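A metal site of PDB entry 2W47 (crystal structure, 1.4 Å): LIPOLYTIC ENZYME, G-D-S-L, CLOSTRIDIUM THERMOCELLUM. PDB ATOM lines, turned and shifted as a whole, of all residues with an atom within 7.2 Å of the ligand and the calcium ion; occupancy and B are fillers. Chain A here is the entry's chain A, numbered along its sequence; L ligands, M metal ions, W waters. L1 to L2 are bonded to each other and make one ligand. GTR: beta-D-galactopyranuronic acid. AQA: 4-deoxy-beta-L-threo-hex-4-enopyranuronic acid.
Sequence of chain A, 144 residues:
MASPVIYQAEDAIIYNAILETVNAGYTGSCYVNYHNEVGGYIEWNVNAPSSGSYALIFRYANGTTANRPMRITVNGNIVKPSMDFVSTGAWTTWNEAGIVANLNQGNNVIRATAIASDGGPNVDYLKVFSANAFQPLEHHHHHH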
ATOM      1  N   GLU A  20      -1.534 -31.037   7.781  1.00  0.00           N
ATOM      2  CA  GLU A  20      -0.246 -30.590   8.314  1.00  0.00           C
ATOM      3  C   GLU A  20      -0.343 -29.177   8.861  1.00  0.00           C
ATOM      4  O   GLU A  20      -1.381 -28.506   8.743  1.00  0.00           O
ATOM      5  CB  GLU A  20       0.859 -30.722   7.270  1.00  0.00           C
ATOM      6  CG  GLU A  20       0.812 -29.701   6.162  1.00  0.00           C
ATOM      7  CD  GLU A  20       2.001 -29.759   5.232  1.00  0.00           C
ATOM      8  OE1 GLU A  20       2.305 -28.700   4.644  1.00  0.00           O
ATOM      9  OE2 GLU A  20       2.627 -30.841   5.076  1.00  0.00           O
ATOM     10  N   VAL A  22       2.775 -27.126   8.736  1.00  0.00           N
ATOM     11  CA  VAL A  22       4.102 -26.614   8.376  1.00  0.00           C
ATOM     12  C   VAL A  22       4.164 -25.108   8.123  1.00  0.00           C
ATOM     13  O   VAL A  22       5.003 -24.410   8.702  1.00  0.00           O
ATOM     14  CB  VAL A  22       4.662 -27.368   7.146  1.00  0.00           C
ATOM     15  CG1 VAL A  22       6.007 -26.783   6.693  1.00  0.00           C
ATOM     16  CG2 VAL A  22       4.804 -28.842   7.469  1.00  0.00           C
ATOM     17  N   ASN A  23       3.278 -24.611   7.272  1.00  0.00           N
ATOM     18  CA  ASN A  23       3.326 -23.220   6.843  1.00  0.00           C
ATOM     19  C   ASN A  23       2.365 -22.347   7.617  1.00  0.00           C
ATOM     20  O   ASN A  23       1.173 -22.640   7.680  1.00  0.00           O
ATOM     21  CB  ASN A  23       3.009 -23.135   5.353  1.00  0.00           C
ATOM     22  CG  ASN A  23       3.997 -23.875   4.503  1.00  0.00           C
ATOM     23  OD1 ASN A  23       3.652 -24.832   3.809  1.00  0.00           O
ATOM     24  ND2 ASN A  23       5.265 -23.467   4.584  1.00  0.00           N
ATOM     25  N   TYR A  31      -4.185 -27.563   7.991  1.00  0.00           N
ATOM     26  CA  TYR A  31      -4.657 -27.419   6.616  1.00  0.00           C
ATOM     27  C   TYR A  31      -4.311 -28.684   5.851  1.00  0.00           C
ATOM     28  O   TYR A  31      -3.551 -29.535   6.346  1.00  0.00           O
ATOM     29  CB  TYR A  31      -4.030 -26.175   5.971  1.00  0.00           C
ATOM     30  CG  TYR A  31      -2.521 -26.233   5.871  1.00  0.00           C
ATOM     31  CD1 TYR A  31      -1.894 -26.836   4.781  1.00  0.00           C
ATOM     32  CD2 TYR A  31      -1.713 -25.676   6.872  1.00  0.00           C
ATOM     33  CE1 TYR A  31      -0.503 -26.894   4.685  1.00  0.00           C
ATOM     34  CE2 TYR A  31      -0.318 -25.718   6.782  1.00  0.00           C
ATOM     35  CZ  TYR A  31       0.276 -26.319   5.675  1.00  0.00           C
ATOM     36  OH  TYR A  31       1.640 -26.368   5.603  1.00  0.00           O
ATOM     37  N   VAL A  32      -4.869 -28.818   4.657  1.00  0.00           N
ATOM     38  CA  VAL A  32      -4.585 -29.974   3.800  1.00  0.00           C
ATOM     39  C   VAL A  32      -3.430 -29.692   2.854  1.00  0.00           C
ATOM     40  O   VAL A  32      -3.389 -28.663   2.192  1.00  0.00           O
ATOM     41  CB  VAL A  32      -5.808 -30.362   2.947  1.00  0.00           C
ATOM     42  CG1 VAL A  32      -5.499 -31.627   2.156  1.00  0.00           C
ATOM     43  CG2 VAL A  32      -7.023 -30.581   3.820  1.00  0.00           C
ATOM     44  N   ASN A  33      -2.486 -30.628   2.800  1.00  0.00           N
ATOM     45  CA  ASN A  33      -1.418 -30.630   1.819  1.00  0.00           C
ATOM     46  C   ASN A  33      -1.587 -31.876   0.953  1.00  0.00           C
ATOM     47  O   ASN A  33      -1.453 -32.985   1.448  1.00  0.00           O
ATOM     48  CB  ASN A  33      -0.065 -30.600   2.538  1.00  0.00           C
ATOM     49  CG  ASN A  33       1.119 -30.846   1.602  1.00  0.00           C
ATOM     50  OD1 ASN A  33       0.996 -30.853   0.384  1.00  0.00           O
ATOM     51  ND2 ASN A  33       2.276 -31.083   2.213  1.00  0.00           N
ATOM     52  N   TYR A  34      -1.926 -31.663  -0.322  1.00  0.00           N
ATOM     53  CA  TYR A  34      -2.116 -32.750  -1.266  1.00  0.00           C
ATOM     54  C   TYR A  34      -0.796 -33.460  -1.539  1.00  0.00           C
ATOM     55  O   TYR A  34       0.249 -32.806  -1.574  1.00  0.00           O
ATOM     56  CB  TYR A  34      -2.607 -32.184  -2.600  1.00  0.00           C
ATOM     57  CG  TYR A  34      -4.071 -31.792  -2.670  1.00  0.00           C
ATOM     58  CD1 TYR A  34      -4.557 -30.646  -2.050  1.00  0.00           C
ATOM     59  CD2 TYR A  34      -4.963 -32.545  -3.429  1.00  0.00           C
ATOM     60  CE1 TYR A  34      -5.888 -30.277  -2.139  1.00  0.00           C
ATOM     61  CE2 TYR A  34      -6.313 -32.188  -3.540  1.00  0.00           C
ATOM     62  CZ  TYR A  34      -6.757 -31.054  -2.881  1.00  0.00           C
ATOM     63  OH  TYR A  34      -8.084 -30.669  -2.964  1.00  0.00           O
ATOM     64  N   HIS A  35      -0.827 -34.768  -1.754  1.00  0.00           N
ATOM     65  CA  HIS A  35       0.343 -35.426  -2.348  1.00  0.00           C
ATOM     66  C   HIS A  35       0.643 -34.756  -3.682  1.00  0.00           C
ATOM     67  O   HIS A  35      -0.278 -34.332  -4.396  1.00  0.00           O
ATOM     68  CB  HIS A  35       0.059 -36.904  -2.615  1.00  0.00           C
ATOM     69  CG  HIS A  35      -0.006 -37.756  -1.391  1.00  0.00           C
ATOM     70  ND1 HIS A  35       0.094 -37.251  -0.112  1.00  0.00           N
ATOM     71  CD2 HIS A  35      -0.192 -39.094  -1.244  1.00  0.00           C
ATOM     72  CE1 HIS A  35      -0.013 -38.236   0.759  1.00  0.00           C
ATOM     73  NE2 HIS A  35      -0.195 -39.370   0.095  1.00  0.00           N
ATOM     74  N   ASN A  36       1.925 -34.675  -4.024  1.00  0.00           N
ATOM     75  CA  ASN A  36       2.305 -34.075  -5.293  1.00  0.00           C
ATOM     76  C   ASN A  36       2.179 -35.088  -6.423  1.00  0.00           C
ATOM     77  O   ASN A  36       3.163 -35.674  -6.900  1.00  0.00           O
ATOM     78  CB  ASN A  36       3.653 -33.375  -5.175  1.00  0.00           C
ATOM     79  CG  ASN A  36       3.574 -32.111  -4.309  1.00  0.00           C
ATOM     80  OD1 ASN A  36       2.834 -32.069  -3.312  1.00  0.00           O
ATOM     81  ND2 ASN A  36       4.287 -31.072  -4.706  1.00  0.00           N
ATOM     82  N   GLU A  37       0.932 -35.319  -6.791  1.00  0.00           N
ATOM     83  CA  GLU A  37       0.559 -36.274  -7.815  1.00  0.00           C
ATOM     84  C   GLU A  37      -0.852 -35.971  -8.318  1.00  0.00           C
ATOM     85  O   GLU A  37      -1.604 -35.227  -7.673  1.00  0.00           O
ATOM     86  CB  GLU A  37       0.634 -37.709  -7.269  1.00  0.00           C
ATOM     87  CG  GLU A  37      -0.380 -38.028  -6.172  1.00  0.00           C
ATOM     88  CD  GLU A  37      -0.178 -39.402  -5.567  1.00  0.00           C
ATOM     89  OE1 GLU A  37       0.894 -39.666  -4.997  1.00  0.00           O
ATOM     90  OE2 GLU A  37      -1.122 -40.220  -5.655  1.00  0.00           O
ATOM     91  N   ALA A  61      -3.213 -21.823  -0.309  1.00  0.00           N
ATOM     92  CA  ALA A  61      -1.908 -21.280  -0.607  1.00  0.00           C
ATOM     93  C   ALA A  61      -1.289 -22.063  -1.736  1.00  0.00           C
ATOM     94  O   ALA A  61      -1.497 -23.270  -1.868  1.00  0.00           O
ATOM     95  CB  ALA A  61      -1.002 -21.310   0.633  1.00  0.00           C
ATOM     96  N   ASN A  62      -0.523 -21.380  -2.571  1.00  0.00           N
ATOM     97  CA  ASN A  62       0.207 -22.013  -3.662  1.00  0.00           C
ATOM     98  C   ASN A  62       1.528 -21.273  -3.813  1.00  0.00           C
ATOM     99  O   ASN A  62       1.604 -20.216  -4.453  1.00  0.00           O
ATOM    100  CB  ASN A  62      -0.602 -22.015  -4.958  1.00  0.00           C
ATOM    101  CG  ASN A  62       0.148 -22.636  -6.119  1.00  0.00           C
ATOM    102  OD1 ASN A  62       1.289 -23.079  -5.962  1.00  0.00           O
ATOM    103  ND2 ASN A  62      -0.481 -22.657  -7.299  1.00  0.00           N
ATOM    104  N   GLY A  63       2.570 -21.843  -3.212  1.00  0.00           N
ATOM    105  CA  GLY A  63       3.891 -21.211  -3.192  1.00  0.00           C
ATOM    106  C   GLY A  63       4.751 -21.573  -4.393  1.00  0.00           C
ATOM    107  O   GLY A  63       5.953 -21.323  -4.373  1.00  0.00           O
ATOM    108  N   THR A  64       4.133 -22.156  -5.410  1.00  0.00           N
ATOM    109  CA  THR A  64       4.819 -22.349  -6.692  1.00  0.00           C
ATOM    110  C   THR A  64       4.300 -21.318  -7.681  1.00  0.00           C
ATOM    111  O   THR A  64       3.294 -20.666  -7.446  1.00  0.00           O
ATOM    112  CB  THR A  64       4.601 -23.767  -7.280  1.00  0.00           C
ATOM    113  OG1 THR A  64       3.302 -23.848  -7.891  1.00  0.00           O
ATOM    114  CG2 THR A  64       4.760 -24.867  -6.215  1.00  0.00           C
ATOM    115  N   ARG A  68      -2.456 -24.674  -9.932  1.00  0.00           N
ATOM    116  CA  ARG A  68      -2.766 -26.037  -9.486  1.00  0.00           C
ATOM    117  C   ARG A  68      -4.273 -26.247  -9.619  1.00  0.00           C
ATOM    118  O   ARG A  68      -5.019 -26.136  -8.633  1.00  0.00           O
ATOM    119  CB  ARG A  68      -2.315 -26.250  -8.041  1.00  0.00           C
ATOM    120  CG  ARG A  68      -0.798 -26.322  -7.925  1.00  0.00           C
ATOM    121  CD  ARG A  68      -0.356 -26.739  -6.537  1.00  0.00           C
ATOM    122  NE  ARG A  68       1.086 -27.044  -6.496  1.00  0.00           N
ATOM    123  CZ  ARG A  68       1.691 -27.523  -5.422  1.00  0.00           C
ATOM    124  NH1 ARG A  68       1.010 -27.744  -4.300  1.00  0.00           N
ATOM    125  NH2 ARG A  68       2.994 -27.780  -5.467  1.00  0.00           N
ATOM    126  N   TRP A  91       4.206 -19.789   0.439  1.00  0.00           N
ATOM    127  CA  TRP A  91       3.426 -20.841   1.090  1.00  0.00           C
ATOM    128  C   TRP A  91       2.700 -20.334   2.331  1.00  0.00           C
ATOM    129  O   TRP A  91       1.788 -20.988   2.835  1.00  0.00           O
ATOM    130  CB  TRP A  91       4.300 -22.051   1.449  1.00  0.00           C
ATOM    131  CG  TRP A  91       4.650 -22.857   0.247  1.00  0.00           C
ATOM    132  CD1 TRP A  91       5.887 -23.009  -0.312  1.00  0.00           C
ATOM    133  CD2 TRP A  91       3.748 -23.614  -0.575  1.00  0.00           C
ATOM    134  NE1 TRP A  91       5.822 -23.814  -1.424  1.00  0.00           N
ATOM    135  CE2 TRP A  91       4.519 -24.211  -1.603  1.00  0.00           C
ATOM    136  CE3 TRP A  91       2.369 -23.866  -0.537  1.00  0.00           C
ATOM    137  CZ2 TRP A  91       3.953 -25.022  -2.589  1.00  0.00           C
ATOM    138  CZ3 TRP A  91       1.810 -24.684  -1.526  1.00  0.00           C
ATOM    139  CH2 TRP A  91       2.599 -25.242  -2.536  1.00  0.00           C
ATOM    140  N   ASP A 118       1.631 -31.936  -9.917  1.00  0.00           N
ATOM    141  CA  ASP A 118       2.158 -31.361  -8.692  1.00  0.00           C
ATOM    142  C   ASP A 118       1.077 -31.319  -7.597  1.00  0.00           C
ATOM    143  O   ASP A 118       1.330 -30.808  -6.513  1.00  0.00           O
ATOM    144  CB  ASP A 118       2.736 -29.961  -8.930  1.00  0.00           C
ATOM    145  CG  ASP A 118       3.924 -29.646  -8.032  1.00  0.00           C
ATOM    146  OD1 ASP A 118       4.540 -30.573  -7.459  1.00  0.00           O
ATOM    147  OD2 ASP A 118       4.240 -28.448  -7.909  1.00  0.00           O
ATOM    148  N   GLY A 119      -0.092 -31.883  -7.882  1.00  0.00           N
ATOM    149  CA  GLY A 119      -1.177 -31.954  -6.900  1.00  0.00           C
ATOM    150  C   GLY A 119      -1.966 -30.674  -6.743  1.00  0.00           C
ATOM    151  O   GLY A 119      -1.890 -29.768  -7.594  1.00  0.00           O
ATOM    152  N   GLY A 120      -2.752 -30.610  -5.681  1.00  0.00           N
ATOM    153  CA  GLY A 120      -3.592 -29.439  -5.419  1.00  0.00           C
ATOM    154  C   GLY A 120      -2.863 -28.417  -4.571  1.00  0.00           C
ATOM    155  O   GLY A 120      -1.785 -28.708  -4.034  1.00  0.00           O
ATOM    156  N   PRO A 121      -3.461 -27.221  -4.429  1.00  0.00           N
ATOM    157  CA  PRO A 121      -2.901 -26.217  -3.536  1.00  0.00           C
ATOM    158  C   PRO A 121      -3.050 -26.708  -2.088  1.00  0.00           C
ATOM    159  O   PRO A 121      -3.814 -27.642  -1.823  1.00  0.00           O
ATOM    160  CB  PRO A 121      -3.828 -25.015  -3.750  1.00  0.00           C
ATOM    161  CG  PRO A 121      -5.141 -25.624  -4.111  1.00  0.00           C
ATOM    162  CD  PRO A 121      -4.753 -26.784  -4.999  1.00  0.00           C
ATOM    163  N   ASN A 122      -2.332 -26.070  -1.170  1.00  0.00           N
ATOM    164  CA  ASN A 122      -2.630 -26.282   0.243  1.00  0.00           C
ATOM    165  C   ASN A 122      -3.963 -25.610   0.553  1.00  0.00           C
ATOM    166  O   ASN A 122      -4.205 -24.479   0.109  1.00  0.00           O
ATOM    167  CB  ASN A 122      -1.532 -25.724   1.127  1.00  0.00           C
ATOM    168  CG  ASN A 122      -0.271 -26.558   1.082  1.00  0.00           C
ATOM    169  OD1 ASN A 122      -0.259 -27.687   0.591  1.00  0.00           O
ATOM    170  ND2 ASN A 122       0.821 -25.997   1.602  1.00  0.00           N
HETATM  171  C1  GTR L   1       9.240 -30.832   1.699  1.00  0.00           C
HETATM  172  C2  GTR L   1       7.947 -31.179   0.954  1.00  0.00           C
HETATM  173  C3  GTR L   1       7.840 -30.386  -0.340  1.00  0.00           C
HETATM  174  C4  GTR L   1       8.017 -28.881  -0.080  1.00  0.00           C
HETATM  175  C5  GTR L   1       9.348 -28.658   0.636  1.00  0.00           C
HETATM  176  C6  GTR L   1       9.588 -27.206   0.942  1.00  0.00           C
HETATM  177  O1  GTR L   1      10.374 -31.361   0.983  1.00  0.00           O
HETATM  178  O2  GTR L   1       7.903 -32.583   0.685  1.00  0.00           O
HETATM  179  O3  GTR L   1       6.578 -30.649  -0.980  1.00  0.00           O
HETATM  180  O4  GTR L   1       6.929 -28.405   0.726  1.00  0.00           O
HETATM  181  O5  GTR L   1       9.367 -29.417   1.866  1.00  0.00           O
HETATM  182  O6A GTR L   1       9.795 -26.853   2.127  1.00  0.00           O
HETATM  183  O6B GTR L   1       9.566 -26.378  -0.003  1.00  0.00           O
HETATM  184  O6A AQA L   2       4.539 -28.480  -3.201  1.00  0.00           O
HETATM  185  C6  AQA L   2       3.803 -28.527  -2.177  1.00  0.00           C
HETATM  186  O6B AQA L   2       2.625 -28.964  -2.207  1.00  0.00           O
HETATM  187  C5  AQA L   2       4.292 -28.081  -1.020  1.00  0.00           C
HETATM  188  O5  AQA L   2       5.655 -27.553  -1.036  1.00  0.00           O
HETATM  189  C4  AQA L   2       3.550 -28.096   0.115  1.00  0.00           C
HETATM  190  C3  AQA L   2       4.186 -27.804   1.454  1.00  0.00           C
HETATM  191  O3  AQA L   2       3.226 -27.338   2.413  1.00  0.00           O
HETATM  192  C2  AQA L   2       5.272 -26.746   1.237  1.00  0.00           C
HETATM  193  O2  AQA L   2       5.934 -26.436   2.457  1.00  0.00           O
HETATM  194  C1  AQA L   2       6.284 -27.241   0.211  1.00  0.00           C
HETATM  195 CA    CA M   1       1.235 -30.699  -1.834  1.00  0.00          CA
HETATM  196  O   HOH W   1       6.862 -27.302  -3.940  1.00  0.00           O
HETATM  197  O   HOH W   2       7.388 -24.045   3.075  1.00  0.00           O
HETATM  198  O   HOH W   3      -0.868 -29.280  -1.511  1.00  0.00           O
HETATM  199  O   HOH W   4       3.347 -31.481  -1.131  1.00  0.00           O
HETATM  200  O   HOH W   5       4.623 -31.920   1.006  1.00  0.00           O
HETATM  201  O   HOH W   6       7.103 -30.330  -3.541  1.00  0.00           O
HETATM  202  O   HOH W   7       0.279 -30.738  -3.950  1.00  0.00           O
HETATM  203  O   HOH W   8       7.131 -28.454   3.758  1.00  0.00           O
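The side-chain carboxylate (OE1) of Glu 20 lies within hydrogen-bond range of an oxygen (O3) of AQA L2. An oxygen (O6A) of AQA L2 is in salt-bridge range of the guanidinium group of Arg 68. An oxygen (O3) of AQA L2 sits at hydrogen-bond distance from the side-chain amide nitrogen (ND2) of Asn 122 (2.9 Å). The side-chain amide oxygen of Asn 23 lies within hydrogen-bond range of an oxygen (O3) of AQA L2 (2.9 Å).
The side-chain amide nitrogen of Asn 33 sits at hydrogen-bond distance from the side-chain carboxylate of Glu 20 (2.9 Å). The side-chain amide oxygen of Asn 122 lies close to the side-chain amide oxygen of Asn 33 (3.4 Å). ND2 of Asn 36 is in hydrogen-bond range of OD1 of Asp 118. The guanidinium group of Arg 68 lies within hydrogen-bond range of the backbone carbonyl oxygen of Gly 120. NH2 of Arg 68 lies within salt-bridge range of OD2 of Asp 118 (2.8 Å). The backbone carbonyl oxygen of Asn 122 is in hydrogen-bond range of the backbone NH of Ala 61 (2.9 Å). N of Asn 23 is in hydrogen-bond range of OH of Tyr 31. OH of Tyr 31 sits at hydrogen-bond distance from N of Val 22 (3.4 Å).
OH of Tyr 31 touches O3 of AQA L2, 3.7 Å away. CZ2 of Trp 91 touches O5 of AQA L2 (3.4 Å). Within 4 Å of the ligand: Glu 20, Asn 23, Tyr 31, Asn 33, Asn 36, Arg 68, Trp 91 and Asn 122. Along chain A the residues within 4 Å of the ligand span positions 20 to 122.
Arg 68 touches the calcium ion (NH1 to CA, 3.9 Å). Of the 21 residues printed, 4 come within 4 Å of the calcium ion.
The calcium ion is bound by the side-chain amide oxygen of Asn 33 (2.2 Å), an oxygen (O6B) of AQA L2 (2.3 Å), water W7 (2.3 Å), the backbone carbonyl oxygen of Tyr 34 (2.3 Å), water W4 (2.4 Å), water W3 (2.6 Å) and the side-chain amide oxygen of Asn 36 (2.6 Å). The calcium ion has seven donor atoms within binding distance.
Water W7 lies within hydrogen-bond range of O of Asp 118 (2.8 Å), O of Gly 120 (2.9 Å) and NH1 of Arg 68 (3.1 Å). Water W6 bridges O3 of GTR L1 and ND2 of Asn 36. Water W2 lies within hydrogen-bond range of the side-chain amide nitrogen (ND2) of Asn 23 (2.7 Å) and an oxygen (O2) of AQA L2 (2.9 Å). Water W5 lies within hydrogen-bond range of the side-chain amide nitrogen of Asn 33 (2.8 Å) and an oxygen (O3) of GTR L1 (3.1 Å).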
